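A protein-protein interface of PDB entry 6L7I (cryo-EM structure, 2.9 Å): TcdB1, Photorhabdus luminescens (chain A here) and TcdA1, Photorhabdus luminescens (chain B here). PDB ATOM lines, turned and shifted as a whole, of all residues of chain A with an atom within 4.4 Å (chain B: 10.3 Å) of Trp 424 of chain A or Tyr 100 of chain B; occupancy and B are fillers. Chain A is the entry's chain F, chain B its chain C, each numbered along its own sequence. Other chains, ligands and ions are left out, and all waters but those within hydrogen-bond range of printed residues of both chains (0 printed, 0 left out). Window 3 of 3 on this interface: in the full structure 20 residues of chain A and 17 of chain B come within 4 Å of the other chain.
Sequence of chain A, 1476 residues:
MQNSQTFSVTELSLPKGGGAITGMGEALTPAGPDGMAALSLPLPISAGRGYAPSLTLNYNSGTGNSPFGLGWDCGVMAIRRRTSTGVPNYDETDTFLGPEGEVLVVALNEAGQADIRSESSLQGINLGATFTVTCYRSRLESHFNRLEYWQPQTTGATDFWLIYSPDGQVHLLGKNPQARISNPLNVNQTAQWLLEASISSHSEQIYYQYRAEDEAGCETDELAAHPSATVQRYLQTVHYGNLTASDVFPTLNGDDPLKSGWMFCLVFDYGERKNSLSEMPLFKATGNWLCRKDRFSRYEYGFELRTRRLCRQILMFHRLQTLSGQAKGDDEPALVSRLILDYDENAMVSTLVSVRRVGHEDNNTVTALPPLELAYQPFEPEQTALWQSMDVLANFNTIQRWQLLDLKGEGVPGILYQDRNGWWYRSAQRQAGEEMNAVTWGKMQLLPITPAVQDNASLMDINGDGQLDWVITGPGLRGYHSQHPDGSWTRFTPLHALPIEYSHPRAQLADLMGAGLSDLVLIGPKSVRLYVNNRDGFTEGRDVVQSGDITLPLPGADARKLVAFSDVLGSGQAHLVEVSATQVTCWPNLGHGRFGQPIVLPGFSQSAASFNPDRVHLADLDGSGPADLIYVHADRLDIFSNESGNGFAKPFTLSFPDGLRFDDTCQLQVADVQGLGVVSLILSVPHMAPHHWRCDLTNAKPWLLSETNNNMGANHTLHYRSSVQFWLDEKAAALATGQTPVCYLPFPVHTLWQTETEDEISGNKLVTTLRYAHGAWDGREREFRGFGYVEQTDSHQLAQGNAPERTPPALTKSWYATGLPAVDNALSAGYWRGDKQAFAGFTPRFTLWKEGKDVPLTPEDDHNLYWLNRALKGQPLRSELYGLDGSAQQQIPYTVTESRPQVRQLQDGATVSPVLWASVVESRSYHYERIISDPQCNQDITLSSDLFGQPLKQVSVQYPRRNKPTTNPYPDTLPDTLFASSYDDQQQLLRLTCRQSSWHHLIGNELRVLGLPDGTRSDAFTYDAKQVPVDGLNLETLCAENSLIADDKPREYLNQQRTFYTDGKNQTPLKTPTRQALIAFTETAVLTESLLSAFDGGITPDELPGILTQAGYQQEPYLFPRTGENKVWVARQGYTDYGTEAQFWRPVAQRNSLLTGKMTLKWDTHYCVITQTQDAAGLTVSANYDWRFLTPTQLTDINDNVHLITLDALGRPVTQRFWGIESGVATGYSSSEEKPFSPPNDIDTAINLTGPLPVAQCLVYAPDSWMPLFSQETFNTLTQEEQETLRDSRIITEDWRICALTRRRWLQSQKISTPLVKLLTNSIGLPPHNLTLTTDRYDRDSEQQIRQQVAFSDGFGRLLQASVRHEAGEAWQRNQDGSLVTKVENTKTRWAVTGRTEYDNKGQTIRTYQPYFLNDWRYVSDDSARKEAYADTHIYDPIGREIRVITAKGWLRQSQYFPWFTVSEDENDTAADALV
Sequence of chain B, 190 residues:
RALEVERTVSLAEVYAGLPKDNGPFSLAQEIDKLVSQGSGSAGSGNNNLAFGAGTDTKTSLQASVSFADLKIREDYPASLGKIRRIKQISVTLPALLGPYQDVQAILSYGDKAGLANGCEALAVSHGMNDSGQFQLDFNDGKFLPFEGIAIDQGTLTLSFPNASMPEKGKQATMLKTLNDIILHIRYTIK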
ATOM      1  N   ILE A 415     -17.521  31.630  -7.186  1.00  0.00           N
ATOM      2  CA  ILE A 415     -16.853  30.380  -7.521  1.00  0.00           C
ATOM      3  C   ILE A 415     -16.049  29.952  -6.309  1.00  0.00           C
ATOM      4  O   ILE A 415     -15.103  30.643  -5.916  1.00  0.00           O
ATOM      5  CB  ILE A 415     -15.945  30.526  -8.750  1.00  0.00           C
ATOM      6  CG1 ILE A 415     -16.711  31.156  -9.909  1.00  0.00           C
ATOM      7  CG2 ILE A 415     -15.404  29.184  -9.156  1.00  0.00           C
ATOM      8  CD1 ILE A 415     -15.865  31.428 -11.111  1.00  0.00           C
ATOM      9  N   LEU A 416     -16.413  28.823  -5.717  1.00  0.00           N
ATOM     10  CA  LEU A 416     -15.720  28.315  -4.543  1.00  0.00           C
ATOM     11  C   LEU A 416     -15.011  27.020  -4.886  1.00  0.00           C
ATOM     12  O   LEU A 416     -15.650  26.047  -5.295  1.00  0.00           O
ATOM     13  CB  LEU A 416     -16.676  28.089  -3.378  1.00  0.00           C
ATOM     14  CG  LEU A 416     -16.043  27.405  -2.170  1.00  0.00           C
ATOM     15  CD1 LEU A 416     -15.094  28.337  -1.474  1.00  0.00           C
ATOM     16  CD2 LEU A 416     -17.104  26.942  -1.218  1.00  0.00           C
ATOM     17  N   TYR A 417     -13.698  27.014  -4.717  1.00  0.00           N
ATOM     18  CA  TYR A 417     -12.903  25.802  -4.692  1.00  0.00           C
ATOM     19  C   TYR A 417     -12.508  25.527  -3.253  1.00  0.00           C
ATOM     20  O   TYR A 417     -12.121  26.441  -2.525  1.00  0.00           O
ATOM     21  CB  TYR A 417     -11.657  25.942  -5.552  1.00  0.00           C
ATOM     22  CG  TYR A 417     -10.829  24.691  -5.632  1.00  0.00           C
ATOM     23  CD1 TYR A 417     -11.293  23.578  -6.309  1.00  0.00           C
ATOM     24  CD2 TYR A 417      -9.579  24.624  -5.042  1.00  0.00           C
ATOM     25  CE1 TYR A 417     -10.538  22.436  -6.400  1.00  0.00           C
ATOM     26  CE2 TYR A 417      -8.816  23.481  -5.129  1.00  0.00           C
ATOM     27  CZ  TYR A 417      -9.307  22.393  -5.808  1.00  0.00           C
ATOM     28  OH  TYR A 417      -8.565  21.247  -5.900  1.00  0.00           O
ATOM     29  N   ASN A 421      -7.684  21.848   3.406  1.00  0.00           N
ATOM     30  CA  ASN A 421      -7.020  22.759   4.326  1.00  0.00           C
ATOM     31  C   ASN A 421      -7.456  24.204   4.128  1.00  0.00           C
ATOM     32  O   ASN A 421      -7.736  24.904   5.103  1.00  0.00           O
ATOM     33  CB  ASN A 421      -5.501  22.649   4.172  1.00  0.00           C
ATOM     34  CG  ASN A 421      -5.028  21.220   4.004  1.00  0.00           C
ATOM     35  OD1 ASN A 421      -4.759  20.523   4.981  1.00  0.00           O
ATOM     36  ND2 ASN A 421      -4.902  20.783   2.758  1.00  0.00           N
ATOM     37  N   GLY A 422      -7.530  24.663   2.881  1.00  0.00           N
ATOM     38  CA  GLY A 422      -7.928  26.025   2.607  1.00  0.00           C
ATOM     39  C   GLY A 422      -8.988  26.076   1.527  1.00  0.00           C
ATOM     40  O   GLY A 422      -9.112  25.172   0.702  1.00  0.00           O
ATOM     41  N   TRP A 423      -9.758  27.158   1.553  1.00  0.00           N
ATOM     42  CA  TRP A 423     -10.817  27.394   0.588  1.00  0.00           C
ATOM     43  C   TRP A 423     -10.464  28.607  -0.251  1.00  0.00           C
ATOM     44  O   TRP A 423      -9.948  29.598   0.267  1.00  0.00           O
ATOM     45  CB  TRP A 423     -12.156  27.637   1.273  1.00  0.00           C
ATOM     46  CG  TRP A 423     -12.765  26.451   1.902  1.00  0.00           C
ATOM     47  CD1 TRP A 423     -12.193  25.237   2.088  1.00  0.00           C
ATOM     48  CD2 TRP A 423     -14.079  26.365   2.447  1.00  0.00           C
ATOM     49  NE1 TRP A 423     -13.069  24.392   2.709  1.00  0.00           N
ATOM     50  CE2 TRP A 423     -14.237  25.063   2.942  1.00  0.00           C
ATOM     51  CE3 TRP A 423     -15.140  27.261   2.560  1.00  0.00           C
ATOM     52  CZ2 TRP A 423     -15.408  24.638   3.546  1.00  0.00           C
ATOM     53  CZ3 TRP A 423     -16.302  26.833   3.155  1.00  0.00           C
ATOM     54  CH2 TRP A 423     -16.427  25.537   3.643  1.00  0.00           C
ATOM     55  N   TRP A 424     -10.756  28.533  -1.541  1.00  0.00           N
ATOM     56  CA  TRP A 424     -10.452  29.609  -2.470  1.00  0.00           C
ATOM     57  C   TRP A 424     -11.751  30.115  -3.072  1.00  0.00           C
ATOM     58  O   TRP A 424     -12.579  29.318  -3.519  1.00  0.00           O
ATOM     59  CB  TRP A 424      -9.501  29.130  -3.562  1.00  0.00           C
ATOM     60  CG  TRP A 424      -8.167  28.702  -3.062  1.00  0.00           C
ATOM     61  CD1 TRP A 424      -7.857  27.514  -2.486  1.00  0.00           C
ATOM     62  CD2 TRP A 424      -6.953  29.455  -3.106  1.00  0.00           C
ATOM     63  NE1 TRP A 424      -6.528  27.479  -2.160  1.00  0.00           N
ATOM     64  CE2 TRP A 424      -5.951  28.660  -2.532  1.00  0.00           C
ATOM     65  CE3 TRP A 424      -6.619  30.729  -3.570  1.00  0.00           C
ATOM     66  CZ2 TRP A 424      -4.639  29.094  -2.410  1.00  0.00           C
ATOM     67  CZ3 TRP A 424      -5.318  31.157  -3.447  1.00  0.00           C
ATOM     68  CH2 TRP A 424      -4.344  30.344  -2.874  1.00  0.00           C
ATOM     69  N   TYR A 425     -11.924  31.431  -3.095  1.00  0.00           N
ATOM     70  CA  TYR A 425     -13.180  32.035  -3.509  1.00  0.00           C
ATOM     71  C   TYR A 425     -12.948  33.052  -4.615  1.00  0.00           C
ATOM     72  O   TYR A 425     -11.868  33.631  -4.737  1.00  0.00           O
ATOM     73  CB  TYR A 425     -13.875  32.707  -2.332  1.00  0.00           C
ATOM     74  CG  TYR A 425     -15.337  32.978  -2.554  1.00  0.00           C
ATOM     75  CD1 TYR A 425     -16.151  32.035  -3.159  1.00  0.00           C
ATOM     76  CD2 TYR A 425     -15.908  34.175  -2.152  1.00  0.00           C
ATOM     77  CE1 TYR A 425     -17.492  32.282  -3.362  1.00  0.00           C
ATOM     78  CE2 TYR A 425     -17.244  34.426  -2.350  1.00  0.00           C
ATOM     79  CZ  TYR A 425     -18.028  33.478  -2.955  1.00  0.00           C
ATOM     80  OH  TYR A 425     -19.357  33.733  -3.152  1.00  0.00           O
ATOM     81  N   MET A 444      -8.846  34.483  -7.525  1.00  0.00           N
ATOM     82  CA  MET A 444      -8.984  33.422  -6.541  1.00  0.00           C
ATOM     83  C   MET A 444      -8.365  33.900  -5.240  1.00  0.00           C
ATOM     84  O   MET A 444      -7.145  34.056  -5.145  1.00  0.00           O
ATOM     85  CB  MET A 444      -8.316  32.147  -7.034  1.00  0.00           C
ATOM     86  CG  MET A 444      -9.103  31.457  -8.109  1.00  0.00           C
ATOM     87  SD  MET A 444     -10.380  30.405  -7.411  1.00  0.00           S
ATOM     88  CE  MET A 444      -9.447  28.915  -7.217  1.00  0.00           C
ATOM     89  N   GLN A 445      -9.202  34.164  -4.249  1.00  0.00           N
ATOM     90  CA  GLN A 445      -8.766  34.696  -2.969  1.00  0.00           C
ATOM     91  C   GLN A 445      -8.819  33.592  -1.930  1.00  0.00           C
ATOM     92  O   GLN A 445      -9.807  32.860  -1.846  1.00  0.00           O
ATOM     93  CB  GLN A 445      -9.642  35.871  -2.540  1.00  0.00           C
ATOM     94  CG  GLN A 445      -9.632  37.034  -3.509  1.00  0.00           C
ATOM     95  CD  GLN A 445      -8.455  37.955  -3.288  1.00  0.00           C
ATOM     96  OE1 GLN A 445      -7.726  37.821  -2.307  1.00  0.00           O
ATOM     97  NE2 GLN A 445      -8.264  38.901  -4.199  1.00  0.00           N
ATOM     98  N   LEU A 446      -7.756  33.471  -1.148  1.00  0.00           N
ATOM     99  CA  LEU A 446      -7.706  32.480  -0.086  1.00  0.00           C
ATOM    100  C   LEU A 446      -8.531  32.963   1.095  1.00  0.00           C
ATOM    101  O   LEU A 446      -8.355  34.088   1.565  1.00  0.00           O
ATOM    102  CB  LEU A 446      -6.259  32.237   0.326  1.00  0.00           C
ATOM    103  CG  LEU A 446      -5.920  31.112   1.294  1.00  0.00           C
ATOM    104  CD1 LEU A 446      -6.669  29.846   0.957  1.00  0.00           C
ATOM    105  CD2 LEU A 446      -4.432  30.879   1.248  1.00  0.00           C
ATOM    106  N   LEU B  96     -12.151  27.085  14.396  1.00  0.00           N
ATOM    107  CA  LEU B  96     -12.004  27.804  13.141  1.00  0.00           C
ATOM    108  C   LEU B  96     -10.520  27.998  12.895  1.00  0.00           C
ATOM    109  O   LEU B  96      -9.865  28.767  13.605  1.00  0.00           O
ATOM    110  CB  LEU B  96     -12.725  29.146  13.183  1.00  0.00           C
ATOM    111  CG  LEU B  96     -14.186  29.080  13.598  1.00  0.00           C
ATOM    112  CD1 LEU B  96     -14.651  30.411  14.134  1.00  0.00           C
ATOM    113  CD2 LEU B  96     -15.004  28.663  12.409  1.00  0.00           C
ATOM    114  N   LEU B  97      -9.992  27.299  11.905  1.00  0.00           N
ATOM    115  CA  LEU B  97      -8.569  27.292  11.625  1.00  0.00           C
ATOM    116  C   LEU B  97      -8.244  28.332  10.567  1.00  0.00           C
ATOM    117  O   LEU B  97      -9.126  28.879   9.909  1.00  0.00           O
ATOM    118  CB  LEU B  97      -8.124  25.902  11.167  1.00  0.00           C
ATOM    119  CG  LEU B  97      -7.634  24.989  12.283  1.00  0.00           C
ATOM    120  CD1 LEU B  97      -7.446  23.591  11.761  1.00  0.00           C
ATOM    121  CD2 LEU B  97      -6.343  25.529  12.838  1.00  0.00           C
ATOM    122  N   GLY B  98      -6.954  28.576  10.383  1.00  0.00           N
ATOM    123  CA  GLY B  98      -6.492  29.512   9.388  1.00  0.00           C
ATOM    124  C   GLY B  98      -6.547  28.947   7.987  1.00  0.00           C
ATOM    125  O   GLY B  98      -7.253  27.976   7.708  1.00  0.00           O
ATOM    126  N   PRO B  99      -5.799  29.552   7.064  1.00  0.00           N
ATOM    127  CA  PRO B  99      -5.831  29.049   5.683  1.00  0.00           C
ATOM    128  C   PRO B  99      -5.111  27.726   5.505  1.00  0.00           C
ATOM    129  O   PRO B  99      -5.614  26.859   4.785  1.00  0.00           O
ATOM    130  CB  PRO B  99      -5.171  30.178   4.884  1.00  0.00           C
ATOM    131  CG  PRO B  99      -4.320  30.886   5.860  1.00  0.00           C
ATOM    132  CD  PRO B  99      -4.996  30.778   7.192  1.00  0.00           C
ATOM    133  N   TYR B 100      -3.951  27.532   6.127  1.00  0.00           N
ATOM    134  CA  TYR B 100      -3.221  26.276   5.978  1.00  0.00           C
ATOM    135  C   TYR B 100      -2.610  25.843   7.299  1.00  0.00           C
ATOM    136  O   TYR B 100      -1.471  25.372   7.350  1.00  0.00           O
ATOM    137  CB  TYR B 100      -2.150  26.391   4.897  1.00  0.00           C
ATOM    138  CG  TYR B 100      -2.712  26.202   3.518  1.00  0.00           C
ATOM    139  CD1 TYR B 100      -3.073  24.946   3.077  1.00  0.00           C
ATOM    140  CD2 TYR B 100      -2.898  27.278   2.663  1.00  0.00           C
ATOM    141  CE1 TYR B 100      -3.610  24.757   1.822  1.00  0.00           C
ATOM    142  CE2 TYR B 100      -3.431  27.100   1.401  1.00  0.00           C
ATOM    143  CZ  TYR B 100      -3.783  25.834   0.989  1.00  0.00           C
ATOM    144  OH  TYR B 100      -4.313  25.632  -0.257  1.00  0.00           O
ATOM    145  N   GLN B 101      -3.359  25.984   8.383  1.00  0.00           N
ATOM    146  CA  GLN B 101      -2.857  25.672   9.711  1.00  0.00           C
ATOM    147  C   GLN B 101      -3.379  24.325  10.184  1.00  0.00           C
ATOM    148  O   GLN B 101      -4.354  23.786   9.658  1.00  0.00           O
ATOM    149  CB  GLN B 101      -3.247  26.760  10.709  1.00  0.00           C
ATOM    150  CG  GLN B 101      -2.902  28.157  10.266  1.00  0.00           C
ATOM    151  CD  GLN B 101      -1.415  28.368  10.117  1.00  0.00           C
ATOM    152  OE1 GLN B 101      -0.952  28.944   9.134  1.00  0.00           O
ATOM    153  NE2 GLN B 101      -0.653  27.909  11.100  1.00  0.00           N
ATOM    154  N   ASP B 102      -2.709  23.786  11.193  1.00  0.00           N
ATOM    155  CA  ASP B 102      -3.062  22.516  11.801  1.00  0.00           C
ATOM    156  C   ASP B 102      -3.305  22.717  13.288  1.00  0.00           C
ATOM    157  O   ASP B 102      -3.034  23.780  13.852  1.00  0.00           O
ATOM    158  CB  ASP B 102      -1.956  21.476  11.591  1.00  0.00           C
ATOM    159  CG  ASP B 102      -1.484  21.408  10.159  1.00  0.00           C
ATOM    160  OD1 ASP B 102      -2.331  21.365   9.248  1.00  0.00           O
ATOM    161  OD2 ASP B 102      -0.259  21.403   9.941  1.00  0.00           O
ATOM    162  N   VAL B 103      -3.814  21.671  13.924  1.00  0.00           N
ATOM    163  CA  VAL B 103      -4.019  21.644  15.364  1.00  0.00           C
ATOM    164  C   VAL B 103      -2.904  20.817  15.980  1.00  0.00           C
ATOM    165  O   VAL B 103      -2.584  19.734  15.480  1.00  0.00           O
ATOM    166  CB  VAL B 103      -5.393  21.056  15.714  1.00  0.00           C
ATOM    167  CG1 VAL B 103      -5.694  21.273  17.165  1.00  0.00           C
ATOM    168  CG2 VAL B 103      -6.461  21.670  14.855  1.00  0.00           C
ATOM    169  N   GLN B 104      -2.294  21.325  17.045  1.00  0.00           N
ATOM    170  CA  GLN B 104      -1.289  20.585  17.797  1.00  0.00           C
ATOM    171  C   GLN B 104      -1.818  20.314  19.196  1.00  0.00           C
ATOM    172  O   GLN B 104      -2.091  21.249  19.950  1.00  0.00           O
ATOM    173  CB  GLN B 104       0.035  21.342  17.865  1.00  0.00           C
ATOM    174  CG  GLN B 104       0.855  21.231  16.608  1.00  0.00           C
ATOM    175  CD  GLN B 104       0.857  22.499  15.796  1.00  0.00           C
ATOM    176  OE1 GLN B 104       0.782  23.595  16.341  1.00  0.00           O
ATOM    177  NE2 GLN B 104       0.933  22.358  14.483  1.00  0.00           N
ATOM    178  N   SER B 125      -3.653  16.019  15.165  1.00  0.00           N
ATOM    179  CA  SER B 125      -3.128  16.780  14.040  1.00  0.00           C
ATOM    180  C   SER B 125      -4.188  17.542  13.265  1.00  0.00           C
ATOM    181  O   SER B 125      -3.913  18.641  12.791  1.00  0.00           O
ATOM    182  CB  SER B 125      -2.370  15.858  13.085  1.00  0.00           C
ATOM    183  OG  SER B 125      -1.521  14.979  13.800  1.00  0.00           O
ATOM    184  N   LYS B 170       1.636  30.414  18.712  1.00  0.00           N
ATOM    185  CA  LYS B 170       0.933  30.333  17.437  1.00  0.00           C
ATOM    186  C   LYS B 170      -0.469  29.759  17.573  1.00  0.00           C
ATOM    187  O   LYS B 170      -1.303  29.988  16.692  1.00  0.00           O
ATOM    188  CB  LYS B 170       1.731  29.499  16.438  1.00  0.00           C
ATOM    189  CG  LYS B 170       2.470  28.335  17.055  1.00  0.00           C
ATOM    190  CD  LYS B 170       3.275  27.578  16.011  1.00  0.00           C
ATOM    191  CE  LYS B 170       2.376  26.797  15.076  1.00  0.00           C
ATOM    192  NZ  LYS B 170       3.155  26.077  14.042  1.00  0.00           N
ATOM    193  N   MET B 174      -6.330  29.990  17.554  1.00  0.00           N
ATOM    194  CA  MET B 174      -7.231  28.868  17.315  1.00  0.00           C
ATOM    195  C   MET B 174      -8.038  28.523  18.554  1.00  0.00           C
ATOM    196  O   MET B 174      -9.198  28.120  18.443  1.00  0.00           O
ATOM    197  CB  MET B 174      -6.436  27.647  16.861  1.00  0.00           C
ATOM    198  CG  MET B 174      -7.276  26.510  16.316  1.00  0.00           C
ATOM    199  SD  MET B 174      -7.661  25.226  17.525  1.00  0.00           S
ATOM    200  CE  MET B 174      -6.033  24.848  18.151  1.00  0.00           C
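The backbone NH of Gly 422 of chain A sits close to the backbone carbonyl oxygen of Pro 99 of chain B, at 3.5 Å. OH of Tyr 100 of chain B sits at hydrogen-bond distance from NE1 of Trp 424 of chain A, at 3.5 Å. O of Pro 99 of chain B sits close to O of Asn 421 of chain A.
N of Trp 424 of chain A lies within hydrogen-bond range of O of Tyr 417 of chain A (2.7 Å).
Among the printed residues, pairs that only touch across the chains: Asn 421 of chain A with Tyr 100 of chain B, Leu 446 of chain A with Pro 99 of chain B and Leu 446 of chain A with Tyr 100 of chain B.
Of chain B, only Tyr 100 comes within 4 Å of Trp 424 of chain A. Of chain A, only Asn 421 (3.5 Å), Trp 424 (3.5 Å) and Leu 446 (3.9 Å) come within 4 Å of Tyr 100 of chain B. Of chain B, only Pro 99 and Tyr 100 come within 4 Å of Asn 421 of chain A. Of chain B, only Pro 99 comes within 4 Å of Gly 422 of chain A. No residue of chain B comes within 4 Å of Met 444 of chain A. Of the printed residues of chain B, Leu 446 of chain A touches Pro 99 (3.8 Å) and Tyr 100 (3.9 Å). Of the printed residues of chain A, Pro 99 of chain B touches Asn 421, Gly 422 and Leu 446. The nearest residue of chain A that does not touch Tyr 100 of chain B is Gly 422 of chain A (4.1 Å). The nearest printed residue of chain B that does not touch Leu 446 of chain A is Gly 98 of chain B (7.0 Å).
Hydrophobic or aromatic side chains of chain A that line the printed part of chain B: Trp 424 and Leu 446. Hydrophobic or aromatic side chains of chain B within 4 Å of the printed part of chain A: Pro 99 and Tyr 100. Among the printed residues, no Asp or Glu carboxylate lies within 4 Å of a Lys or Arg side-chain nitrogen of the other chain.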
